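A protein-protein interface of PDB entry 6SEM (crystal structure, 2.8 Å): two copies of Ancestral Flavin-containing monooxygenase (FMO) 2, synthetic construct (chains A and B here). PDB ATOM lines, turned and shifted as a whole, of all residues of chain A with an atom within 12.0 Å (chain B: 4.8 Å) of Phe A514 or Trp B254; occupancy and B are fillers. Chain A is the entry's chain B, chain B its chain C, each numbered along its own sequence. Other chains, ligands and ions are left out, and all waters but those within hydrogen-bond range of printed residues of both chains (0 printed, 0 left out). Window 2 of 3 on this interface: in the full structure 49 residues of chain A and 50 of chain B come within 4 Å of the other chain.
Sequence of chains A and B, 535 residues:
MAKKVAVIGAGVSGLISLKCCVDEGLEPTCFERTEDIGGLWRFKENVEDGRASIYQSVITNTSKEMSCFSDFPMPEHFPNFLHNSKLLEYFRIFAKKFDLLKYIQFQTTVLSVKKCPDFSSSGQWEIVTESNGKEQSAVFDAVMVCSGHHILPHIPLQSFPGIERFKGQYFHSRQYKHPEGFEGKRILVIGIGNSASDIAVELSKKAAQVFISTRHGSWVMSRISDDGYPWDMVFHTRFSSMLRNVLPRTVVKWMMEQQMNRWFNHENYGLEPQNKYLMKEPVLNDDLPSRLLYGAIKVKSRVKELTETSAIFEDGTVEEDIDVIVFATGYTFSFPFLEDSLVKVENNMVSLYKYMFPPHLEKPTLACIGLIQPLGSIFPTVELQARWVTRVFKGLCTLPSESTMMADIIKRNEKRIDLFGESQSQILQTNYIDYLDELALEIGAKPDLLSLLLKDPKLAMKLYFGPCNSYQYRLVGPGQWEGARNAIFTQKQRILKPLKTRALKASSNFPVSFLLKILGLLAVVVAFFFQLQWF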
ATOM      1  N   ASP A 227     -19.232  12.695  38.643  1.00  0.00           N
ATOM      2  CA  ASP A 227     -18.721  13.872  37.920  1.00  0.00           C
ATOM      3  C   ASP A 227     -17.420  14.378  38.563  1.00  0.00           C
ATOM      4  O   ASP A 227     -17.032  15.557  38.391  1.00  0.00           O
ATOM      5  CB  ASP A 227     -19.804  14.949  37.830  1.00  0.00           C
ATOM      6  CG  ASP A 227     -21.038  14.487  37.074  1.00  0.00           C
ATOM      7  OD1 ASP A 227     -20.899  14.173  35.884  1.00  0.00           O
ATOM      8  OD2 ASP A 227     -22.122  14.417  37.682  1.00  0.00           O
ATOM      9  N   ALA A 506     -14.880  29.090  25.733  1.00  0.00           N
ATOM     10  CA  ALA A 506     -15.695  28.541  24.635  1.00  0.00           C
ATOM     11  C   ALA A 506     -17.157  28.477  25.087  1.00  0.00           C
ATOM     12  O   ALA A 506     -17.462  27.739  26.014  1.00  0.00           O
ATOM     13  CB  ALA A 506     -15.237  27.152  24.234  1.00  0.00           C
ATOM     14  N   SER A 507     -18.030  29.246  24.421  1.00  0.00           N
ATOM     15  CA  SER A 507     -19.493  29.213  24.617  1.00  0.00           C
ATOM     16  C   SER A 507     -20.086  28.117  23.720  1.00  0.00           C
ATOM     17  O   SER A 507     -20.318  28.340  22.533  1.00  0.00           O
ATOM     18  CB  SER A 507     -20.111  30.576  24.336  1.00  0.00           C
ATOM     19  OG  SER A 507     -21.332  30.756  25.045  1.00  0.00           O
ATOM     20  N   SER A 508     -20.323  26.935  24.306  1.00  0.00           N
ATOM     21  CA  SER A 508     -20.604  25.705  23.558  1.00  0.00           C
ATOM     22  C   SER A 508     -22.099  25.597  23.203  1.00  0.00           C
ATOM     23  O   SER A 508     -22.959  25.478  24.088  1.00  0.00           O
ATOM     24  CB  SER A 508     -20.113  24.501  24.323  1.00  0.00           C
ATOM     25  OG  SER A 508     -20.672  24.450  25.628  1.00  0.00           O
ATOM     26  N   ASN A 509     -22.381  25.642  21.891  1.00  0.00           N
ATOM     27  CA  ASN A 509     -23.730  25.557  21.287  1.00  0.00           C
ATOM     28  C   ASN A 509     -23.779  24.371  20.313  1.00  0.00           C
ATOM     29  O   ASN A 509     -24.575  23.440  20.503  1.00  0.00           O
ATOM     30  CB  ASN A 509     -24.107  26.844  20.539  1.00  0.00           C
ATOM     31  CG  ASN A 509     -24.433  28.010  21.449  1.00  0.00           C
ATOM     32  OD1 ASN A 509     -23.658  28.960  21.557  1.00  0.00           O
ATOM     33  ND2 ASN A 509     -25.579  27.948  22.105  1.00  0.00           N
ATOM     34  N   PHE A 510     -22.910  24.430  19.286  1.00  0.00           N
ATOM     35  CA  PHE A 510     -22.871  23.478  18.146  1.00  0.00           C
ATOM     36  C   PHE A 510     -21.835  22.367  18.376  1.00  0.00           C
ATOM     37  O   PHE A 510     -22.192  21.196  18.264  1.00  0.00           O
ATOM     38  CB  PHE A 510     -22.689  24.186  16.790  1.00  0.00           C
ATOM     39  CG  PHE A 510     -22.324  25.656  16.788  1.00  0.00           C
ATOM     40  CD1 PHE A 510     -23.225  26.620  17.227  1.00  0.00           C
ATOM     41  CD2 PHE A 510     -21.100  26.090  16.287  1.00  0.00           C
ATOM     42  CE1 PHE A 510     -22.892  27.968  17.212  1.00  0.00           C
ATOM     43  CE2 PHE A 510     -20.769  27.439  16.272  1.00  0.00           C
ATOM     44  CZ  PHE A 510     -21.666  28.377  16.733  1.00  0.00           C
ATOM     45  N   PRO A 511     -20.534  22.645  18.672  1.00  0.00           N
ATOM     46  CA  PRO A 511     -19.551  21.575  18.871  1.00  0.00           C
ATOM     47  C   PRO A 511     -19.804  20.635  20.064  1.00  0.00           C
ATOM     48  O   PRO A 511     -19.583  19.434  19.932  1.00  0.00           O
ATOM     49  CB  PRO A 511     -18.220  22.313  19.103  1.00  0.00           C
ATOM     50  CG  PRO A 511     -18.447  23.684  18.515  1.00  0.00           C
ATOM     51  CD  PRO A 511     -19.909  23.974  18.777  1.00  0.00           C
ATOM     52  N   VAL A 512     -20.256  21.172  21.208  1.00  0.00           N
ATOM     53  CA  VAL A 512     -20.305  20.384  22.456  1.00  0.00           C
ATOM     54  C   VAL A 512     -21.234  21.031  23.499  1.00  0.00           C
ATOM     55  O   VAL A 512     -20.765  21.663  24.446  1.00  0.00           O
ATOM     56  CB  VAL A 512     -18.886  20.203  23.030  1.00  0.00           C
ATOM     57  CG1 VAL A 512     -18.150  21.534  23.178  1.00  0.00           C
ATOM     58  CG2 VAL A 512     -18.910  19.431  24.341  1.00  0.00           C
ATOM     59  N   SER A 513     -22.546  20.813  23.359  1.00  0.00           N
ATOM     60  CA  SER A 513     -23.524  21.228  24.372  1.00  0.00           C
ATOM     61  C   SER A 513     -24.632  20.172  24.438  1.00  0.00           C
ATOM     62  O   SER A 513     -25.792  20.456  24.178  1.00  0.00           O
ATOM     63  CB  SER A 513     -24.032  22.636  24.096  1.00  0.00           C
ATOM     64  OG  SER A 513     -25.375  22.663  23.634  1.00  0.00           O
ATOM     65  N   PHE A 514     -24.232  18.957  24.832  1.00  0.00           N
ATOM     66  CA  PHE A 514     -24.981  17.719  24.560  1.00  0.00           C
ATOM     67  C   PHE A 514     -26.391  17.807  25.175  1.00  0.00           C
ATOM     68  O   PHE A 514     -27.355  18.113  24.448  1.00  0.00           O
ATOM     69  CB  PHE A 514     -24.145  16.506  24.997  1.00  0.00           C
ATOM     70  CG  PHE A 514     -24.412  15.203  24.270  1.00  0.00           C
ATOM     71  CD1 PHE A 514     -24.768  15.176  22.928  1.00  0.00           C
ATOM     72  CD2 PHE A 514     -24.254  13.983  24.919  1.00  0.00           C
ATOM     73  CE1 PHE A 514     -24.999  13.970  22.279  1.00  0.00           C
ATOM     74  CE2 PHE A 514     -24.477  12.777  24.262  1.00  0.00           C
ATOM     75  CZ  PHE A 514     -24.851  12.773  22.941  1.00  0.00           C
ATOM     76  N   LEU A 515     -26.515  17.595  26.499  1.00  0.00           N
ATOM     77  CA  LEU A 515     -27.826  17.475  27.174  1.00  0.00           C
ATOM     78  C   LEU A 515     -28.333  18.871  27.578  1.00  0.00           C
ATOM     79  O   LEU A 515     -29.060  19.011  28.563  1.00  0.00           O
ATOM     80  CB  LEU A 515     -27.707  16.529  28.382  1.00  0.00           C
ATOM     81  CG  LEU A 515     -27.314  15.081  28.060  1.00  0.00           C
ATOM     82  CD1 LEU A 515     -25.813  14.865  28.200  1.00  0.00           C
ATOM     83  CD2 LEU A 515     -28.072  14.086  28.934  1.00  0.00           C
ATOM     84  N   LEU A 516     -27.956  19.893  26.790  1.00  0.00           N
ATOM     85  CA  LEU A 516     -28.441  21.271  26.951  1.00  0.00           C
ATOM     86  C   LEU A 516     -29.820  21.404  26.283  1.00  0.00           C
ATOM     87  O   LEU A 516     -30.803  21.784  26.938  1.00  0.00           O
ATOM     88  CB  LEU A 516     -27.411  22.254  26.374  1.00  0.00           C
ATOM     89  CG  LEU A 516     -26.248  22.599  27.315  1.00  0.00           C
ATOM     90  CD1 LEU A 516     -25.277  21.434  27.452  1.00  0.00           C
ATOM     91  CD2 LEU A 516     -25.520  23.859  26.868  1.00  0.00           C
ATOM     92  N   LYS A 517     -29.887  21.050  24.993  1.00  0.00           N
ATOM     93  CA  LYS A 517     -31.127  21.091  24.199  1.00  0.00           C
ATOM     94  C   LYS A 517     -31.889  19.756  24.304  1.00  0.00           C
ATOM     95  O   LYS A 517     -33.107  19.713  24.074  1.00  0.00           O
ATOM     96  CB  LYS A 517     -30.832  21.406  22.729  1.00  0.00           C
ATOM     97  CG  LYS A 517     -29.928  22.608  22.463  1.00  0.00           C
ATOM     98  CD  LYS A 517     -28.461  22.281  22.268  1.00  0.00           C
ATOM     99  CE  LYS A 517     -28.207  21.231  21.206  1.00  0.00           C
ATOM    100  NZ  LYS A 517     -28.307  19.852  21.742  1.00  0.00           N
ATOM    101  N   ILE A 518     -31.177  18.665  24.625  1.00  0.00           N
ATOM    102  CA  ILE A 518     -31.791  17.327  24.853  1.00  0.00           C
ATOM    103  C   ILE A 518     -32.625  17.355  26.148  1.00  0.00           C
ATOM    104  O   ILE A 518     -33.551  16.582  26.308  1.00  0.00           O
ATOM    105  CB  ILE A 518     -30.717  16.215  24.845  1.00  0.00           C
ATOM    106  CG1 ILE A 518     -30.283  15.883  23.412  1.00  0.00           C
ATOM    107  CG2 ILE A 518     -31.185  14.971  25.594  1.00  0.00           C
ATOM    108  CD1 ILE A 518     -29.474  14.615  23.272  1.00  0.00           C
ATOM    109  N   LEU A 519     -32.275  18.252  27.069  1.00  0.00           N
ATOM    110  CA  LEU A 519     -33.055  18.535  28.292  1.00  0.00           C
ATOM    111  C   LEU A 519     -34.227  19.477  27.972  1.00  0.00           C
ATOM    112  O   LEU A 519     -35.334  19.248  28.426  1.00  0.00           O
ATOM    113  CB  LEU A 519     -32.129  19.124  29.363  1.00  0.00           C
ATOM    114  CG  LEU A 519     -31.761  18.168  30.500  1.00  0.00           C
ATOM    115  CD1 LEU A 519     -30.713  18.786  31.417  1.00  0.00           C
ATOM    116  CD2 LEU A 519     -33.003  17.769  31.290  1.00  0.00           C
ATOM    117  N   GLY A 520     -33.957  20.542  27.210  1.00  0.00           N
ATOM    118  CA  GLY A 520     -34.979  21.460  26.686  1.00  0.00           C
ATOM    119  C   GLY A 520     -36.089  20.728  25.932  1.00  0.00           C
ATOM    120  O   GLY A 520     -37.282  21.042  26.077  1.00  0.00           O
ATOM    121  N   LEU A 521     -35.685  19.726  25.137  1.00  0.00           N
ATOM    122  CA  LEU A 521     -36.561  18.920  24.260  1.00  0.00           C
ATOM    123  C   LEU A 521     -37.470  17.993  25.081  1.00  0.00           C
ATOM    124  O   LEU A 521     -38.684  18.057  24.947  1.00  0.00           O
ATOM    125  CB  LEU A 521     -35.691  18.122  23.278  1.00  0.00           C
ATOM    126  CG  LEU A 521     -36.426  17.086  22.423  1.00  0.00           C
ATOM    127  CD1 LEU A 521     -36.033  17.213  20.959  1.00  0.00           C
ATOM    128  CD2 LEU A 521     -36.169  15.669  22.917  1.00  0.00           C
ATOM    129  N   LEU A 522     -36.879  17.125  25.908  1.00  0.00           N
ATOM    130  CA  LEU A 522     -37.615  16.093  26.687  1.00  0.00           C
ATOM    131  C   LEU A 522     -38.538  16.752  27.727  1.00  0.00           C
ATOM    132  O   LEU A 522     -39.521  16.147  28.129  1.00  0.00           O
ATOM    133  CB  LEU A 522     -36.620  15.125  27.346  1.00  0.00           C
ATOM    134  CG  LEU A 522     -37.030  13.648  27.446  1.00  0.00           C
ATOM    135  CD1 LEU A 522     -38.355  13.460  28.176  1.00  0.00           C
ATOM    136  CD2 LEU A 522     -37.083  12.982  26.076  1.00  0.00           C
ATOM    137  N   ALA A 523     -38.218  17.977  28.160  1.00  0.00           N
ATOM    138  CA  ALA A 523     -39.056  18.771  29.085  1.00  0.00           C
ATOM    139  C   ALA A 523     -40.250  19.380  28.338  1.00  0.00           C
ATOM    140  O   ALA A 523     -41.364  19.391  28.853  1.00  0.00           O
ATOM    141  CB  ALA A 523     -38.229  19.843  29.746  1.00  0.00           C
ATOM    142  N   THR B 250     -19.323  12.902  14.916  1.00  0.00           N
ATOM    143  CA  THR B 250     -19.844  13.567  16.114  1.00  0.00           C
ATOM    144  C   THR B 250     -20.517  12.535  17.025  1.00  0.00           C
ATOM    145  O   THR B 250     -20.113  12.386  18.162  1.00  0.00           O
ATOM    146  CB  THR B 250     -20.800  14.710  15.771  1.00  0.00           C
ATOM    147  OG1 THR B 250     -21.578  14.235  14.676  1.00  0.00           O
ATOM    148  CG2 THR B 250     -20.086  16.000  15.427  1.00  0.00           C
ATOM    149  N   VAL B 251     -21.503  11.799  16.508  1.00  0.00           N
ATOM    150  CA  VAL B 251     -22.168  10.758  17.294  1.00  0.00           C
ATOM    151  C   VAL B 251     -21.129   9.952  18.075  1.00  0.00           C
ATOM    152  O   VAL B 251     -21.419   9.522  19.180  1.00  0.00           O
ATOM    153  CB  VAL B 251     -23.005   9.821  16.412  1.00  0.00           C
ATOM    154  CG1 VAL B 251     -23.230   8.454  17.049  1.00  0.00           C
ATOM    155  CG2 VAL B 251     -24.331  10.458  16.041  1.00  0.00           C
ATOM    156  N   VAL B 252     -19.961   9.711  17.468  1.00  0.00           N
ATOM    157  CA  VAL B 252     -18.899   8.941  18.097  1.00  0.00           C
ATOM    158  C   VAL B 252     -18.231   9.799  19.175  1.00  0.00           C
ATOM    159  O   VAL B 252     -18.062   9.348  20.289  1.00  0.00           O
ATOM    160  CB  VAL B 252     -17.883   8.429  17.058  1.00  0.00           C
ATOM    161  CG1 VAL B 252     -16.604   7.934  17.707  1.00  0.00           C
ATOM    162  CG2 VAL B 252     -18.471   7.338  16.187  1.00  0.00           C
ATOM    163  N   LYS B 253     -17.851  11.028  18.826  1.00  0.00           N
ATOM    164  CA  LYS B 253     -17.285  11.998  19.780  1.00  0.00           C
ATOM    165  C   LYS B 253     -18.257  12.216  20.953  1.00  0.00           C
ATOM    166  O   LYS B 253     -17.838  12.202  22.099  1.00  0.00           O
ATOM    167  CB  LYS B 253     -16.947  13.298  19.041  1.00  0.00           C
ATOM    168  CG  LYS B 253     -17.141  14.589  19.821  1.00  0.00           C
ATOM    169  CD  LYS B 253     -17.560  15.780  18.960  1.00  0.00           C
ATOM    170  CE  LYS B 253     -17.646  17.088  19.727  1.00  0.00           C
ATOM    171  NZ  LYS B 253     -18.795  17.139  20.671  1.00  0.00           N
ATOM    172  N   TRP B 254     -19.544  12.425  20.646  1.00  0.00           N
ATOM    173  CA  TRP B 254     -20.635  12.583  21.642  1.00  0.00           C
ATOM    174  C   TRP B 254     -20.612  11.422  22.631  1.00  0.00           C
ATOM    175  O   TRP B 254     -21.088  11.552  23.729  1.00  0.00           O
ATOM    176  CB  TRP B 254     -22.025  12.615  20.986  1.00  0.00           C
ATOM    177  CG  TRP B 254     -22.433  13.870  20.271  1.00  0.00           C
ATOM    178  CD1 TRP B 254     -21.719  15.025  20.113  1.00  0.00           C
ATOM    179  CD2 TRP B 254     -23.630  14.036  19.484  1.00  0.00           C
ATOM    180  NE1 TRP B 254     -22.426  15.927  19.362  1.00  0.00           N
ATOM    181  CE2 TRP B 254     -23.595  15.343  18.945  1.00  0.00           C
ATOM    182  CE3 TRP B 254     -24.735  13.218  19.208  1.00  0.00           C
ATOM    183  CZ2 TRP B 254     -24.624  15.843  18.146  1.00  0.00           C
ATOM    184  CZ3 TRP B 254     -25.752  13.715  18.421  1.00  0.00           C
ATOM    185  CH2 TRP B 254     -25.693  15.010  17.896  1.00  0.00           C
ATOM    186  N   MET B 255     -20.164  10.263  22.159  1.00  0.00           N
ATOM    187  CA  MET B 255     -20.153   9.035  22.925  1.00  0.00           C
ATOM    188  C   MET B 255     -18.851   8.925  23.714  1.00  0.00           C
ATOM    189  O   MET B 255     -18.878   8.606  24.882  1.00  0.00           O
ATOM    190  CB  MET B 255     -20.338   7.817  22.018  1.00  0.00           C
ATOM    191  CG  MET B 255     -21.826   7.558  21.762  1.00  0.00           C
ATOM    192  SD  MET B 255     -22.205   6.326  20.515  1.00  0.00           S
ATOM    193  CE  MET B 255     -23.685   5.590  21.217  1.00  0.00           C
ATOM    194  N   MET B 256     -17.715   9.193  23.074  1.00  0.00           N
ATOM    195  CA  MET B 256     -16.442   9.218  23.790  1.00  0.00           C
ATOM    196  C   MET B 256     -16.602  10.181  24.968  1.00  0.00           C
ATOM    197  O   MET B 256     -16.387   9.808  26.108  1.00  0.00           O
ATOM    198  CB  MET B 256     -15.258   9.656  22.912  1.00  0.00           C
ATOM    199  CG  MET B 256     -14.032   8.745  23.032  1.00  0.00           C
ATOM    200  SD  MET B 256     -14.035   7.297  21.905  1.00  0.00           S
ATOM    201  CE  MET B 256     -15.232   6.215  22.690  1.00  0.00           C
ATOM    202  N   GLU B 257     -17.044  11.402  24.684  1.00  0.00           N
ATOM    203  CA  GLU B 257     -17.170  12.439  25.696  1.00  0.00           C
ATOM    204  C   GLU B 257     -17.887  11.880  26.937  1.00  0.00           C
ATOM    205  O   GLU B 257     -17.394  12.009  28.051  1.00  0.00           O
ATOM    206  CB  GLU B 257     -17.883  13.661  25.106  1.00  0.00           C
ATOM    207  CG  GLU B 257     -17.931  14.843  26.049  1.00  0.00           C
ATOM    208  CD  GLU B 257     -18.022  16.220  25.416  1.00  0.00           C
ATOM    209  OE1 GLU B 257     -17.696  16.351  24.207  1.00  0.00           O
ATOM    210  OE2 GLU B 257     -18.444  17.143  26.141  1.00  0.00           O
ATOM    211  N   GLN B 258     -19.037  11.233  26.730  1.00  0.00           N
ATOM    212  CA  GLN B 258     -19.849  10.720  27.829  1.00  0.00           C
ATOM    213  C   GLN B 258     -19.067   9.627  28.553  1.00  0.00           C
ATOM    214  O   GLN B 258     -18.753   9.764  29.726  1.00  0.00           O
ATOM    215  CB  GLN B 258     -21.214  10.213  27.342  1.00  0.00           C
ATOM    216  CG  GLN B 258     -22.390  11.108  27.735  1.00  0.00           C
ATOM    217  CD  GLN B 258     -22.216  12.578  27.410  1.00  0.00           C
ATOM    218  OE1 GLN B 258     -21.495  12.968  26.486  1.00  0.00           O
ATOM    219  NE2 GLN B 258     -22.900  13.420  28.174  1.00  0.00           N
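The backbone carbonyl oxygen of Pro A511 sits at hydrogen-bond distance from the side-chain amino group of Lys B253 (2.5 Å).
O of Phe A514 lies within hydrogen-bond range of NZ of Lys A517, at 3.4 Å. The backbone carbonyl oxygen (O) of Trp B254 sits close to the side-chain amide oxygen (OE1) of Gln B258 (3.1 Å). The side-chain hydroxyl of Ser A508 lies close to the backbone carbonyl oxygen of Val A512 (3.0 Å). The side-chain carboxylate (OE1) of Glu B257 is in salt-bridge range of the side-chain amino group (NZ) of Lys B253.
Among the printed residues, merely in contact across the chains: Val A512 with Glu B257, Phe A514 with Trp B254, Leu A515 with Gln B258, Phe A514 with Gln B258 and Val A512 with Lys B253.
Printed residues of chain B within 4 Å of Pro A511: Lys B253 (2.5 Å). Of the printed residues of chain B, Val A512 touches Lys B253 and Glu B257. Of chain B, only Trp B254 (3.1 Å) and Gln B258 (3.3 Å) come within 4 Å of Phe A514. Of the printed residues of chain B, Leu A515 touches Gln B258. Leu A521 touches none of the printed residues of chain B. Ala A523 touches none of the printed residues of chain B. Val B251 touches none of the printed residues of chain A. Of chain A, only Pro A511 (2.5 Å) and Val A512 (3.9 Å) come within 4 Å of Lys B253. Trp B254 touches one residue of chain A. No residue of chain A comes within 4 Å of Met B255. The nearest printed residue of chain B that does not touch Phe A514 is Met B255 (5.4 Å).
Of the 9 printed residues of chain B, 4 touch a printed residue of chain A. Hydrophobic or aromatic side chains of chain B within 4 Å of the printed part of chain A: Trp B254. Printed residues of chain A that touch a printed residue of chain B: Pro A511, Val A512, Phe A514 and Leu A515.
No position is printed for both chains. Of the 6 pairs that touch across the chains among the printed residues, none has its exchanged pair printed and touching as well.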
